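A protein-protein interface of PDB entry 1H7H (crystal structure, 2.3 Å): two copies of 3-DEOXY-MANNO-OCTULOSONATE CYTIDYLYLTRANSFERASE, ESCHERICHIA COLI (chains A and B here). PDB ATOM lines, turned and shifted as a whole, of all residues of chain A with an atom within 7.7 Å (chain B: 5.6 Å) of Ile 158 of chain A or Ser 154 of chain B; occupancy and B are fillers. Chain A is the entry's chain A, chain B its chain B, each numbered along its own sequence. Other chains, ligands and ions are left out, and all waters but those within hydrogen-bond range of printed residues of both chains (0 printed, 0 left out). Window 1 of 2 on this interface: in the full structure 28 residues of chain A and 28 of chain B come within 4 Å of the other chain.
Tyr 152 of chain B touches Tyr 152 of chain A (CB to CB, 3.7 Å). Tyr 152 of chain A touches Ile 158 of chain B (CE2 to CG2, 3.9 Å). Ser 154 of chain A touches Ile 158 of chain B. Ile 158 of chain A touches Ser 154 of chain B. Tyr 152 of chain B touches Pro 159 of chain A (OH to CB, 3.4 Å). Pro 159 of chain A touches Glu 198 of chain B. Tyr 160 of chain A touches Arg 155 of chain B. Ser 156 of chain B touches Tyr 160 of chain A (OG to CD1, 3.2 Å).
Tyr 152 of chain A touches its own counterpart, Tyr 152 of chain B. Tyr 152 of chain A touches Ile 158 of chain B, but with the chains exchanged Ile 158 of chain A does not touch Tyr 152 of chain B (4.04 Å). Ser 154 of chain A touches Ile 158 of chain B, and with the chains exchanged Ile 158 of chain A touches Ser 154 of chain B. 10 positions are printed for both chains.
Ala 135 of chain A touches none of the printed residues of chain B. Printed residues of chain B within 4 Å of Ile 158 of chain A: Ser 154 (3.97 Å). Printed residues of chain B within 4 Å of Pro 159 of chain A: Tyr 152 (3.4 Å) and Glu 198 (3.4 Å). Ser 154 of chain B touches just one residue of chain A: Ile 158. Printed residues of chain A within 4 Å of Ser 156 of chain B: Pro 157 (2.7 Å) and Tyr 160 (3.2 Å). The nearest residue of chain B that does not touch Ile 158 of chain A is Tyr 152 of chain B (4.04 Å).
Hydrophobic or aromatic side chains of chain B within 4 Å of the printed part of chain A: Tyr 152 and Ile 158. Of the 24 printed residues of chain A, 6 touch a printed residue of chain B.
OH of Tyr 152 of chain A sits at hydrogen-bond distance from OE2 of Glu 198 of chain A (2.9 Å). The side-chain hydroxyl of Ser 154 of chain A sits at hydrogen-bond distance from the side-chain carboxylate of Glu 198 of chain A, 2.6 Å away. The side-chain hydroxyl (OH) of Tyr 169 of chain A sits at hydrogen-bond distance from the backbone carbonyl oxygen (O) of Pro 159 of chain A, 2.8 Å away. The backbone carbonyl oxygen of Ser 154 of chain B sits at hydrogen-bond distance from the backbone NH of Lys 141 of chain B (2.8 Å). The side-chain amino group of Lys 141 of chain B sits at hydrogen-bond distance from the backbone carbonyl oxygen of Arg 155 of chain B, 2.8 Å away. The side-chain carboxylate (OE2) of Glu 198 of chain B sits at hydrogen-bond distance from the side-chain hydroxyl (OG) of Ser 154 of chain B (2.6 Å).
The backbone carbonyl oxygen (O) of Pro 157 of chain A lies within hydrogen-bond range of the side-chain hydroxyl (OG) of Ser 156 of chain B (2.7 Å). N of Tyr 160 of chain A sits at hydrogen-bond distance from OE2 of Glu 198 of chain B (2.8 Å).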
ATOM      1  N   ILE A 129      14.294 -15.471  -8.955  1.00  0.00           N
ATOM      2  CA  ILE A 129      13.210 -16.286  -9.501  1.00  0.00           C
ATOM      3  C   ILE A 129      13.609 -16.750 -10.902  1.00  0.00           C
ATOM      4  O   ILE A 129      14.528 -16.194 -11.507  1.00  0.00           O
ATOM      5  CB  ILE A 129      11.851 -15.534  -9.573  1.00  0.00           C
ATOM      6  CG1 ILE A 129      12.000 -14.218 -10.322  1.00  0.00           C
ATOM      7  CG2 ILE A 129      11.294 -15.317  -8.181  1.00  0.00           C
ATOM      8  CD1 ILE A 129      10.686 -13.606 -10.731  1.00  0.00           C
ATOM      9  N   ALA A 134       8.934 -15.138 -13.713  1.00  0.00           N
ATOM     10  CA  ALA A 134       9.038 -13.733 -14.086  1.00  0.00           C
ATOM     11  C   ALA A 134       8.043 -13.315 -15.173  1.00  0.00           C
ATOM     12  O   ALA A 134       7.731 -12.132 -15.310  1.00  0.00           O
ATOM     13  CB  ALA A 134      10.446 -13.419 -14.519  1.00  0.00           C
ATOM     14  N   ALA A 135       7.537 -14.279 -15.938  1.00  0.00           N
ATOM     15  CA  ALA A 135       6.578 -13.974 -17.000  1.00  0.00           C
ATOM     16  C   ALA A 135       5.213 -13.500 -16.470  1.00  0.00           C
ATOM     17  O   ALA A 135       4.466 -12.819 -17.180  1.00  0.00           O
ATOM     18  CB  ALA A 135       6.398 -15.183 -17.911  1.00  0.00           C
ATOM     19  N   VAL A 140       6.090  -8.901  -9.297  1.00  0.00           N
ATOM     20  CA  VAL A 140       6.785  -7.650  -9.567  1.00  0.00           C
ATOM     21  C   VAL A 140       8.286  -7.894  -9.680  1.00  0.00           C
ATOM     22  O   VAL A 140       8.899  -8.463  -8.778  1.00  0.00           O
ATOM     23  CB  VAL A 140       6.491  -6.593  -8.461  1.00  0.00           C
ATOM     24  CG1 VAL A 140       7.216  -5.279  -8.753  1.00  0.00           C
ATOM     25  CG2 VAL A 140       4.996  -6.336  -8.368  1.00  0.00           C
ATOM     26  N   LYS A 141       8.862  -7.505 -10.814  1.00  0.00           N
ATOM     27  CA  LYS A 141      10.293  -7.663 -11.049  1.00  0.00           C
ATOM     28  C   LYS A 141      11.018  -6.368 -10.717  1.00  0.00           C
ATOM     29  O   LYS A 141      10.425  -5.286 -10.756  1.00  0.00           O
ATOM     30  CB  LYS A 141      10.574  -8.035 -12.509  1.00  0.00           C
ATOM     31  CG  LYS A 141      10.411  -9.514 -12.843  1.00  0.00           C
ATOM     32  CD  LYS A 141       8.968  -9.981 -12.760  1.00  0.00           C
ATOM     33  CE  LYS A 141       8.068  -9.230 -13.726  1.00  0.00           C
ATOM     34  NZ  LYS A 141       6.720  -9.858 -13.850  1.00  0.00           N
ATOM     35  N   VAL A 142      12.307  -6.490 -10.413  1.00  0.00           N
ATOM     36  CA  VAL A 142      13.139  -5.346 -10.092  1.00  0.00           C
ATOM     37  C   VAL A 142      14.541  -5.569 -10.662  1.00  0.00           C
ATOM     38  O   VAL A 142      15.017  -6.702 -10.734  1.00  0.00           O
ATOM     39  CB  VAL A 142      13.207  -5.104  -8.541  1.00  0.00           C
ATOM     40  CG1 VAL A 142      13.768  -6.322  -7.817  1.00  0.00           C
ATOM     41  CG2 VAL A 142      14.042  -3.874  -8.223  1.00  0.00           C
ATOM     42  N   VAL A 143      15.161  -4.485 -11.132  1.00  0.00           N
ATOM     43  CA  VAL A 143      16.514  -4.517 -11.675  1.00  0.00           C
ATOM     44  C   VAL A 143      17.310  -3.528 -10.831  1.00  0.00           C
ATOM     45  O   VAL A 143      16.851  -2.408 -10.603  1.00  0.00           O
ATOM     46  CB  VAL A 143      16.543  -4.088 -13.166  1.00  0.00           C
ATOM     47  CG1 VAL A 143      17.987  -3.964 -13.653  1.00  0.00           C
ATOM     48  CG2 VAL A 143      15.809  -5.108 -14.010  1.00  0.00           C
ATOM     49  N   VAL A 144      18.501  -3.933 -10.392  1.00  0.00           N
ATOM     50  CA  VAL A 144      19.346  -3.107  -9.530  1.00  0.00           C
ATOM     51  C   VAL A 144      20.723  -2.788 -10.124  1.00  0.00           C
ATOM     52  O   VAL A 144      21.150  -3.441 -11.063  1.00  0.00           O
ATOM     53  CB  VAL A 144      19.558  -3.824  -8.153  1.00  0.00           C
ATOM     54  CG1 VAL A 144      18.211  -4.155  -7.500  1.00  0.00           C
ATOM     55  CG2 VAL A 144      20.369  -5.116  -8.336  1.00  0.00           C
ATOM     56  N   LEU A 151      16.726   0.226 -10.112  1.00  0.00           N
ATOM     57  CA  LEU A 151      16.692   1.058 -11.312  1.00  0.00           C
ATOM     58  C   LEU A 151      15.227   1.219 -11.685  1.00  0.00           C
ATOM     59  O   LEU A 151      14.771   2.312 -11.999  1.00  0.00           O
ATOM     60  CB  LEU A 151      17.447   0.404 -12.472  1.00  0.00           C
ATOM     61  CG  LEU A 151      18.961   0.289 -12.302  1.00  0.00           C
ATOM     62  CD1 LEU A 151      19.555  -0.398 -13.506  1.00  0.00           C
ATOM     63  CD2 LEU A 151      19.572   1.670 -12.129  1.00  0.00           C
ATOM     64  N   TYR A 152      14.469   0.137 -11.580  1.00  0.00           N
ATOM     65  CA  TYR A 152      13.054   0.197 -11.919  1.00  0.00           C
ATOM     66  C   TYR A 152      12.336  -1.066 -11.445  1.00  0.00           C
ATOM     67  O   TYR A 152      12.965  -2.108 -11.267  1.00  0.00           O
ATOM     68  CB  TYR A 152      12.905   0.363 -13.440  1.00  0.00           C
ATOM     69  CG  TYR A 152      11.494   0.609 -13.926  1.00  0.00           C
ATOM     70  CD1 TYR A 152      10.789   1.741 -13.528  1.00  0.00           C
ATOM     71  CD2 TYR A 152      10.854  -0.304 -14.765  1.00  0.00           C
ATOM     72  CE1 TYR A 152       9.476   1.959 -13.942  1.00  0.00           C
ATOM     73  CE2 TYR A 152       9.536  -0.092 -15.187  1.00  0.00           C
ATOM     74  CZ  TYR A 152       8.854   1.041 -14.767  1.00  0.00           C
ATOM     75  OH  TYR A 152       7.549   1.247 -15.159  1.00  0.00           O
ATOM     76  N   PHE A 153      11.032  -0.943 -11.194  1.00  0.00           N
ATOM     77  CA  PHE A 153      10.178  -2.062 -10.767  1.00  0.00           C
ATOM     78  C   PHE A 153       9.129  -2.221 -11.866  1.00  0.00           C
ATOM     79  O   PHE A 153       8.566  -1.223 -12.313  1.00  0.00           O
ATOM     80  CB  PHE A 153       9.418  -1.746  -9.465  1.00  0.00           C
ATOM     81  CG  PHE A 153      10.291  -1.592  -8.249  1.00  0.00           C
ATOM     82  CD1 PHE A 153      10.913  -0.377  -7.970  1.00  0.00           C
ATOM     83  CD2 PHE A 153      10.465  -2.653  -7.365  1.00  0.00           C
ATOM     84  CE1 PHE A 153      11.700  -0.215  -6.821  1.00  0.00           C
ATOM     85  CE2 PHE A 153      11.248  -2.508  -6.212  1.00  0.00           C
ATOM     86  CZ  PHE A 153      11.867  -1.282  -5.943  1.00  0.00           C
ATOM     87  N   SER A 154       8.801  -3.454 -12.251  1.00  0.00           N
ATOM     88  CA  SER A 154       7.805  -3.634 -13.306  1.00  0.00           C
ATOM     89  C   SER A 154       7.133  -4.996 -13.319  1.00  0.00           C
ATOM     90  O   SER A 154       7.662  -5.969 -12.784  1.00  0.00           O
ATOM     91  CB  SER A 154       8.444  -3.380 -14.686  1.00  0.00           C
ATOM     92  OG  SER A 154       7.471  -3.380 -15.721  1.00  0.00           O
ATOM     93  N   ARG A 155       5.937  -5.034 -13.903  1.00  0.00           N
ATOM     94  CA  ARG A 155       5.182  -6.272 -14.053  1.00  0.00           C
ATOM     95  C   ARG A 155       5.655  -6.932 -15.352  1.00  0.00           C
ATOM     96  O   ARG A 155       5.426  -8.121 -15.571  1.00  0.00           O
ATOM     97  CB  ARG A 155       3.678  -5.999 -14.103  1.00  0.00           C
ATOM     98  CG  ARG A 155       3.119  -5.449 -12.800  1.00  0.00           C
ATOM     99  CD  ARG A 155       1.613  -5.241 -12.875  1.00  0.00           C
ATOM    100  NE  ARG A 155       1.113  -4.597 -11.664  1.00  0.00           N
ATOM    101  CZ  ARG A 155       0.853  -5.230 -10.523  1.00  0.00           C
ATOM    102  NH1 ARG A 155       1.028  -6.541 -10.425  1.00  0.00           N
ATOM    103  NH2 ARG A 155       0.483  -4.538  -9.456  1.00  0.00           N
ATOM    104  N   SER A 156       6.312  -6.146 -16.207  1.00  0.00           N
ATOM    105  CA  SER A 156       6.870  -6.652 -17.459  1.00  0.00           C
ATOM    106  C   SER A 156       8.153  -7.394 -17.105  1.00  0.00           C
ATOM    107  O   SER A 156       8.837  -7.046 -16.141  1.00  0.00           O
ATOM    108  CB  SER A 156       7.248  -5.513 -18.414  1.00  0.00           C
ATOM    109  OG  SER A 156       6.117  -4.893 -18.991  1.00  0.00           O
ATOM    110  N   PRO A 157       8.488  -8.444 -17.867  1.00  0.00           N
ATOM    111  CA  PRO A 157       9.719  -9.157 -17.540  1.00  0.00           C
ATOM    112  C   PRO A 157      10.917  -8.272 -17.840  1.00  0.00           C
ATOM    113  O   PRO A 157      11.137  -7.894 -18.994  1.00  0.00           O
ATOM    114  CB  PRO A 157       9.684 -10.355 -18.494  1.00  0.00           C
ATOM    115  CG  PRO A 157       8.220 -10.575 -18.718  1.00  0.00           C
ATOM    116  CD  PRO A 157       7.726  -9.164 -18.902  1.00  0.00           C
ATOM    117  N   ILE A 158      11.627  -7.854 -16.794  1.00  0.00           N
ATOM    118  CA  ILE A 158      12.838  -7.057 -16.973  1.00  0.00           C
ATOM    119  C   ILE A 158      13.946  -7.737 -16.166  1.00  0.00           C
ATOM    120  O   ILE A 158      13.704  -8.230 -15.066  1.00  0.00           O
ATOM    121  CB  ILE A 158      12.685  -5.558 -16.542  1.00  0.00           C
ATOM    122  CG1 ILE A 158      12.223  -5.436 -15.088  1.00  0.00           C
ATOM    123  CG2 ILE A 158      11.765  -4.812 -17.505  1.00  0.00           C
ATOM    124  CD1 ILE A 158      12.283  -4.012 -14.560  1.00  0.00           C
ATOM    125  N   PRO A 159      15.155  -7.845 -16.736  1.00  0.00           N
ATOM    126  CA  PRO A 159      15.526  -7.364 -18.070  1.00  0.00           C
ATOM    127  C   PRO A 159      14.905  -8.203 -19.189  1.00  0.00           C
ATOM    128  O   PRO A 159      14.512  -9.354 -18.970  1.00  0.00           O
ATOM    129  CB  PRO A 159      17.047  -7.485 -18.051  1.00  0.00           C
ATOM    130  CG  PRO A 159      17.265  -8.709 -17.214  1.00  0.00           C
ATOM    131  CD  PRO A 159      16.310  -8.470 -16.064  1.00  0.00           C
ATOM    132  N   TYR A 160      14.757  -7.603 -20.369  1.00  0.00           N
ATOM    133  CA  TYR A 160      14.195  -8.312 -21.515  1.00  0.00           C
ATOM    134  C   TYR A 160      15.169  -9.430 -21.890  1.00  0.00           C
ATOM    135  O   TYR A 160      16.383  -9.221 -21.936  1.00  0.00           O
ATOM    136  CB  TYR A 160      13.999  -7.362 -22.695  1.00  0.00           C
ATOM    137  CG  TYR A 160      13.384  -8.031 -23.901  1.00  0.00           C
ATOM    138  CD1 TYR A 160      12.005  -8.220 -23.986  1.00  0.00           C
ATOM    139  CD2 TYR A 160      14.183  -8.507 -24.940  1.00  0.00           C
ATOM    140  CE1 TYR A 160      11.436  -8.873 -25.075  1.00  0.00           C
ATOM    141  CE2 TYR A 160      13.625  -9.158 -26.031  1.00  0.00           C
ATOM    142  CZ  TYR A 160      12.253  -9.340 -26.091  1.00  0.00           C
ATOM    143  OH  TYR A 160      11.698 -10.002 -27.160  1.00  0.00           O
ATOM    144  N   PRO A 161      14.648 -10.634 -22.164  1.00  0.00           N
ATOM    145  CA  PRO A 161      15.504 -11.768 -22.523  1.00  0.00           C
ATOM    146  C   PRO A 161      15.964 -11.823 -23.990  1.00  0.00           C
ATOM    147  O   PRO A 161      15.575 -12.730 -24.729  1.00  0.00           O
ATOM    148  CB  PRO A 161      14.622 -12.953 -22.169  1.00  0.00           C
ATOM    149  CG  PRO A 161      13.268 -12.469 -22.617  1.00  0.00           C
ATOM    150  CD  PRO A 161      13.229 -11.039 -22.111  1.00  0.00           C
ATOM    151  N   ALA A 167      20.119 -13.630 -18.771  1.00  0.00           N
ATOM    152  CA  ALA A 167      19.146 -12.991 -17.893  1.00  0.00           C
ATOM    153  C   ALA A 167      18.985 -13.653 -16.518  1.00  0.00           C
ATOM    154  O   ALA A 167      18.951 -14.883 -16.395  1.00  0.00           O
ATOM    155  CB  ALA A 167      17.790 -12.903 -18.589  1.00  0.00           C
ATOM    156  N   ARG A 168      18.915 -12.812 -15.489  1.00  0.00           N
ATOM    157  CA  ARG A 168      18.722 -13.258 -14.112  1.00  0.00           C
ATOM    158  C   ARG A 168      17.617 -12.371 -13.545  1.00  0.00           C
ATOM    159  O   ARG A 168      17.701 -11.142 -13.606  1.00  0.00           O
ATOM    160  CB  ARG A 168      20.012 -13.113 -13.300  1.00  0.00           C
ATOM    161  CG  ARG A 168      19.923 -13.709 -11.903  1.00  0.00           C
ATOM    162  CD  ARG A 168      21.262 -13.652 -11.177  1.00  0.00           C
ATOM    163  NE  ARG A 168      21.177 -14.229  -9.834  1.00  0.00           N
ATOM    164  CZ  ARG A 168      20.828 -13.553  -8.739  1.00  0.00           C
ATOM    165  NH1 ARG A 168      20.528 -12.263  -8.808  1.00  0.00           N
ATOM    166  NH2 ARG A 168      20.773 -14.172  -7.570  1.00  0.00           N
ATOM    167  N   TYR A 169      16.563 -13.002 -13.042  1.00  0.00           N
ATOM    168  CA  TYR A 169      15.416 -12.286 -12.503  1.00  0.00           C
ATOM    169  C   TYR A 169      15.334 -12.191 -10.983  1.00  0.00           C
ATOM    170  O   TYR A 169      15.704 -13.124 -10.261  1.00  0.00           O
ATOM    171  CB  TYR A 169      14.122 -12.888 -13.059  1.00  0.00           C
ATOM    172  CG  TYR A 169      14.006 -12.730 -14.551  1.00  0.00           C
ATOM    173  CD1 TYR A 169      13.491 -11.562 -15.101  1.00  0.00           C
ATOM    174  CD2 TYR A 169      14.487 -13.714 -15.420  1.00  0.00           C
ATOM    175  CE1 TYR A 169      13.463 -11.367 -16.476  1.00  0.00           C
ATOM    176  CE2 TYR A 169      14.463 -13.527 -16.800  1.00  0.00           C
ATOM    177  CZ  TYR A 169      13.951 -12.348 -17.318  1.00  0.00           C
ATOM    178  OH  TYR A 169      13.942 -12.126 -18.669  1.00  0.00           O
ATOM    179  N   LEU A 170      14.864 -11.033 -10.517  1.00  0.00           N
ATOM    180  CA  LEU A 170      14.686 -10.757  -9.095  1.00  0.00           C
ATOM    181  C   LEU A 170      13.245 -10.383  -8.859  1.00  0.00           C
ATOM    182  O   LEU A 170      12.684  -9.565  -9.577  1.00  0.00           O
ATOM    183  CB  LEU A 170      15.571  -9.600  -8.634  1.00  0.00           C
ATOM    184  CG  LEU A 170      17.078  -9.866  -8.576  1.00  0.00           C
ATOM    185  CD1 LEU A 170      17.837  -8.556  -8.352  1.00  0.00           C
ATOM    186  CD2 LEU A 170      17.388 -10.882  -7.474  1.00  0.00           C
ATOM    187  N   GLU A 198       1.361   1.003 -14.232  1.00  0.00           N
ATOM    188  CA  GLU A 198       1.737  -0.292 -13.655  1.00  0.00           C
ATOM    189  C   GLU A 198       0.927  -0.685 -12.424  1.00  0.00           C
ATOM    190  O   GLU A 198       0.819  -1.871 -12.092  1.00  0.00           O
ATOM    191  CB  GLU A 198       3.214  -0.268 -13.248  1.00  0.00           C
ATOM    192  CG  GLU A 198       4.194  -0.077 -14.391  1.00  0.00           C
ATOM    193  CD  GLU A 198       5.017  -1.315 -14.665  1.00  0.00           C
ATOM    194  OE1 GLU A 198       4.692  -2.392 -14.124  1.00  0.00           O
ATOM    195  OE2 GLU A 198       5.996  -1.217 -15.424  1.00  0.00           O
ATOM    196  N   THR B 139      12.492  -1.903 -30.781  1.00  0.00           N
ATOM    197  CA  THR B 139      12.325  -0.514 -30.370  1.00  0.00           C
ATOM    198  C   THR B 139      12.715  -0.430 -28.890  1.00  0.00           C
ATOM    199  O   THR B 139      12.200  -1.181 -28.064  1.00  0.00           O
ATOM    200  CB  THR B 139      10.866  -0.051 -30.566  1.00  0.00           C
ATOM    201  OG1 THR B 139      10.611   0.127 -31.962  1.00  0.00           O
ATOM    202  CG2 THR B 139      10.615   1.249 -29.869  1.00  0.00           C
ATOM    203  N   VAL B 140      13.674   0.434 -28.569  1.00  0.00           N
ATOM    204  CA  VAL B 140      14.110   0.593 -27.186  1.00  0.00           C
ATOM    205  C   VAL B 140      13.249   1.621 -26.446  1.00  0.00           C
ATOM    206  O   VAL B 140      13.123   2.779 -26.865  1.00  0.00           O
ATOM    207  CB  VAL B 140      15.606   0.995 -27.092  1.00  0.00           C
ATOM    208  CG1 VAL B 140      16.014   1.181 -25.634  1.00  0.00           C
ATOM    209  CG2 VAL B 140      16.483  -0.077 -27.740  1.00  0.00           C
ATOM    210  N   LYS B 141      12.599   1.166 -25.380  1.00  0.00           N
ATOM    211  CA  LYS B 141      11.767   2.041 -24.566  1.00  0.00           C
ATOM    212  C   LYS B 141      12.551   2.599 -23.377  1.00  0.00           C
ATOM    213  O   LYS B 141      13.518   1.996 -22.903  1.00  0.00           O
ATOM    214  CB  LYS B 141      10.517   1.308 -24.060  1.00  0.00           C
ATOM    215  CG  LYS B 141       9.354   1.233 -25.053  1.00  0.00           C
ATOM    216  CD  LYS B 141       9.644   0.281 -26.193  1.00  0.00           C
ATOM    217  CE  LYS B 141       9.821  -1.142 -25.690  1.00  0.00           C
ATOM    218  NZ  LYS B 141      10.073  -2.106 -26.794  1.00  0.00           N
ATOM    219  N   VAL B 142      12.142   3.775 -22.921  1.00  0.00           N
ATOM    220  CA  VAL B 142      12.776   4.412 -21.780  1.00  0.00           C
ATOM    221  C   VAL B 142      11.687   4.989 -20.878  1.00  0.00           C
ATOM    222  O   VAL B 142      10.615   5.379 -21.358  1.00  0.00           O
ATOM    223  CB  VAL B 142      13.777   5.541 -22.221  1.00  0.00           C
ATOM    224  CG1 VAL B 142      13.052   6.664 -22.961  1.00  0.00           C
ATOM    225  CG2 VAL B 142      14.531   6.090 -21.023  1.00  0.00           C
ATOM    226  N   TYR B 152      15.209   3.458 -16.461  1.00  0.00           N
ATOM    227  CA  TYR B 152      15.661   2.226 -17.098  1.00  0.00           C
ATOM    228  C   TYR B 152      15.364   2.247 -18.599  1.00  0.00           C
ATOM    229  O   TYR B 152      14.492   2.996 -19.055  1.00  0.00           O
ATOM    230  CB  TYR B 152      14.956   1.029 -16.430  1.00  0.00           C
ATOM    231  CG  TYR B 152      15.475  -0.339 -16.830  1.00  0.00           C
ATOM    232  CD1 TYR B 152      16.813  -0.679 -16.648  1.00  0.00           C
ATOM    233  CD2 TYR B 152      14.624  -1.289 -17.403  1.00  0.00           C
ATOM    234  CE1 TYR B 152      17.292  -1.929 -17.029  1.00  0.00           C
ATOM    235  CE2 TYR B 152      15.094  -2.534 -17.785  1.00  0.00           C
ATOM    236  CZ  TYR B 152      16.429  -2.847 -17.598  1.00  0.00           C
ATOM    237  OH  TYR B 152      16.906  -4.076 -17.997  1.00  0.00           O
ATOM    238  N   PHE B 153      16.150   1.478 -19.359  1.00  0.00           N
ATOM    239  CA  PHE B 153      15.978   1.335 -20.817  1.00  0.00           C
ATOM    240  C   PHE B 153      15.686  -0.144 -21.052  1.00  0.00           C
ATOM    241  O   PHE B 153      16.380  -1.001 -20.501  1.00  0.00           O
ATOM    242  CB  PHE B 153      17.263   1.692 -21.571  1.00  0.00           C
ATOM    243  CG  PHE B 153      17.657   3.132 -21.470  1.00  0.00           C
ATOM    244  CD1 PHE B 153      18.424   3.585 -20.396  1.00  0.00           C
ATOM    245  CD2 PHE B 153      17.307   4.030 -22.472  1.00  0.00           C
ATOM    246  CE1 PHE B 153      18.843   4.908 -20.322  1.00  0.00           C
ATOM    247  CE2 PHE B 153      17.724   5.366 -22.409  1.00  0.00           C
ATOM    248  CZ  PHE B 153      18.494   5.802 -21.330  1.00  0.00           C
ATOM    249  N   SER B 154      14.701  -0.457 -21.884  1.00  0.00           N
ATOM    250  CA  SER B 154      14.375  -1.858 -22.113  1.00  0.00           C
ATOM    251  C   SER B 154      13.689  -2.146 -23.448  1.00  0.00           C
ATOM    252  O   SER B 154      13.111  -1.252 -24.078  1.00  0.00           O
ATOM    253  CB  SER B 154      13.486  -2.361 -20.969  1.00  0.00           C
ATOM    254  OG  SER B 154      13.284  -3.763 -21.022  1.00  0.00           O
ATOM    255  N   ARG B 155      13.782  -3.404 -23.875  1.00  0.00           N
ATOM    256  CA  ARG B 155      13.132  -3.858 -25.100  1.00  0.00           C
ATOM    257  C   ARG B 155      11.724  -4.314 -24.721  1.00  0.00           C
ATOM    258  O   ARG B 155      10.876  -4.517 -25.587  1.00  0.00           O
ATOM    259  CB  ARG B 155      13.915  -4.996 -25.758  1.00  0.00           C
ATOM    260  CG  ARG B 155      15.271  -4.566 -26.287  1.00  0.00           C
ATOM    261  CD  ARG B 155      16.001  -5.712 -26.977  1.00  0.00           C
ATOM    262  NE  ARG B 155      17.357  -5.332 -27.361  1.00  0.00           N
ATOM    263  CZ  ARG B 155      17.662  -4.522 -28.376  1.00  0.00           C
ATOM    264  NH1 ARG B 155      16.710  -3.999 -29.138  1.00  0.00           N
ATOM    265  NH2 ARG B 155      18.925  -4.187 -28.592  1.00  0.00           N
ATOM    266  N   SER B 156      11.491  -4.471 -23.415  1.00  0.00           N
ATOM    267  CA  SER B 156      10.178  -4.853 -22.892  1.00  0.00           C
ATOM    268  C   SER B 156       9.303  -3.609 -22.861  1.00  0.00           C
ATOM    269  O   SER B 156       9.801  -2.494 -22.701  1.00  0.00           O
ATOM    270  CB  SER B 156      10.287  -5.404 -21.465  1.00  0.00           C
ATOM    271  OG  SER B 156      10.665  -6.763 -21.451  1.00  0.00           O
ATOM    272  N   ILE B 158       7.713  -0.950 -21.323  1.00  0.00           N
ATOM    273  CA  ILE B 158       7.667  -0.288 -20.020  1.00  0.00           C
ATOM    274  C   ILE B 158       7.210   1.152 -20.245  1.00  0.00           C
ATOM    275  O   ILE B 158       7.679   1.819 -21.166  1.00  0.00           O
ATOM    276  CB  ILE B 158       9.028  -0.315 -19.251  1.00  0.00           C
ATOM    277  CG1 ILE B 158      10.169   0.217 -20.110  1.00  0.00           C
ATOM    278  CG2 ILE B 158       9.336  -1.723 -18.756  1.00  0.00           C
ATOM    279  CD1 ILE B 158      11.482   0.299 -19.359  1.00  0.00           C
ATOM    280  N   GLU B 198      19.670  -7.657 -22.231  1.00  0.00           N
ATOM    281  CA  GLU B 198      18.903  -6.790 -23.127  1.00  0.00           C
ATOM    282  C   GLU B 198      19.660  -6.488 -24.415  1.00  0.00           C
ATOM    283  O   GLU B 198      19.057  -6.255 -25.461  1.00  0.00           O
ATOM    284  CB  GLU B 198      18.617  -5.456 -22.430  1.00  0.00           C
ATOM    285  CG  GLU B 198      17.756  -5.540 -21.181  1.00  0.00           C
ATOM    286  CD  GLU B 198      16.338  -5.040 -21.404  1.00  0.00           C
ATOM    287  OE1 GLU B 198      15.973  -4.773 -22.566  1.00  0.00           O
ATOM    288  OE2 GLU B 198      15.585  -4.917 -20.413  1.00  0.00           O
ATOM    289  N   LEU B 200      21.963  -3.863 -24.612  1.00  0.00           N
ATOM    290  CA  LEU B 200      21.891  -2.399 -24.638  1.00  0.00           C
ATOM    291  C   LEU B 200      23.111  -1.867 -23.881  1.00  0.00           C
ATOM    292  O   LEU B 200      23.185  -1.963 -22.653  1.00  0.00           O
ATOM    293  CB  LEU B 200      20.600  -1.912 -23.959  1.00  0.00           C
ATOM    294  CG  LEU B 200      19.283  -2.244 -24.672  1.00  0.00           C
ATOM    295  CD1 LEU B 200      18.102  -1.825 -23.831  1.00  0.00           C
ATOM    296  CD2 LEU B 200      19.242  -1.560 -26.026  1.00  0.00           C
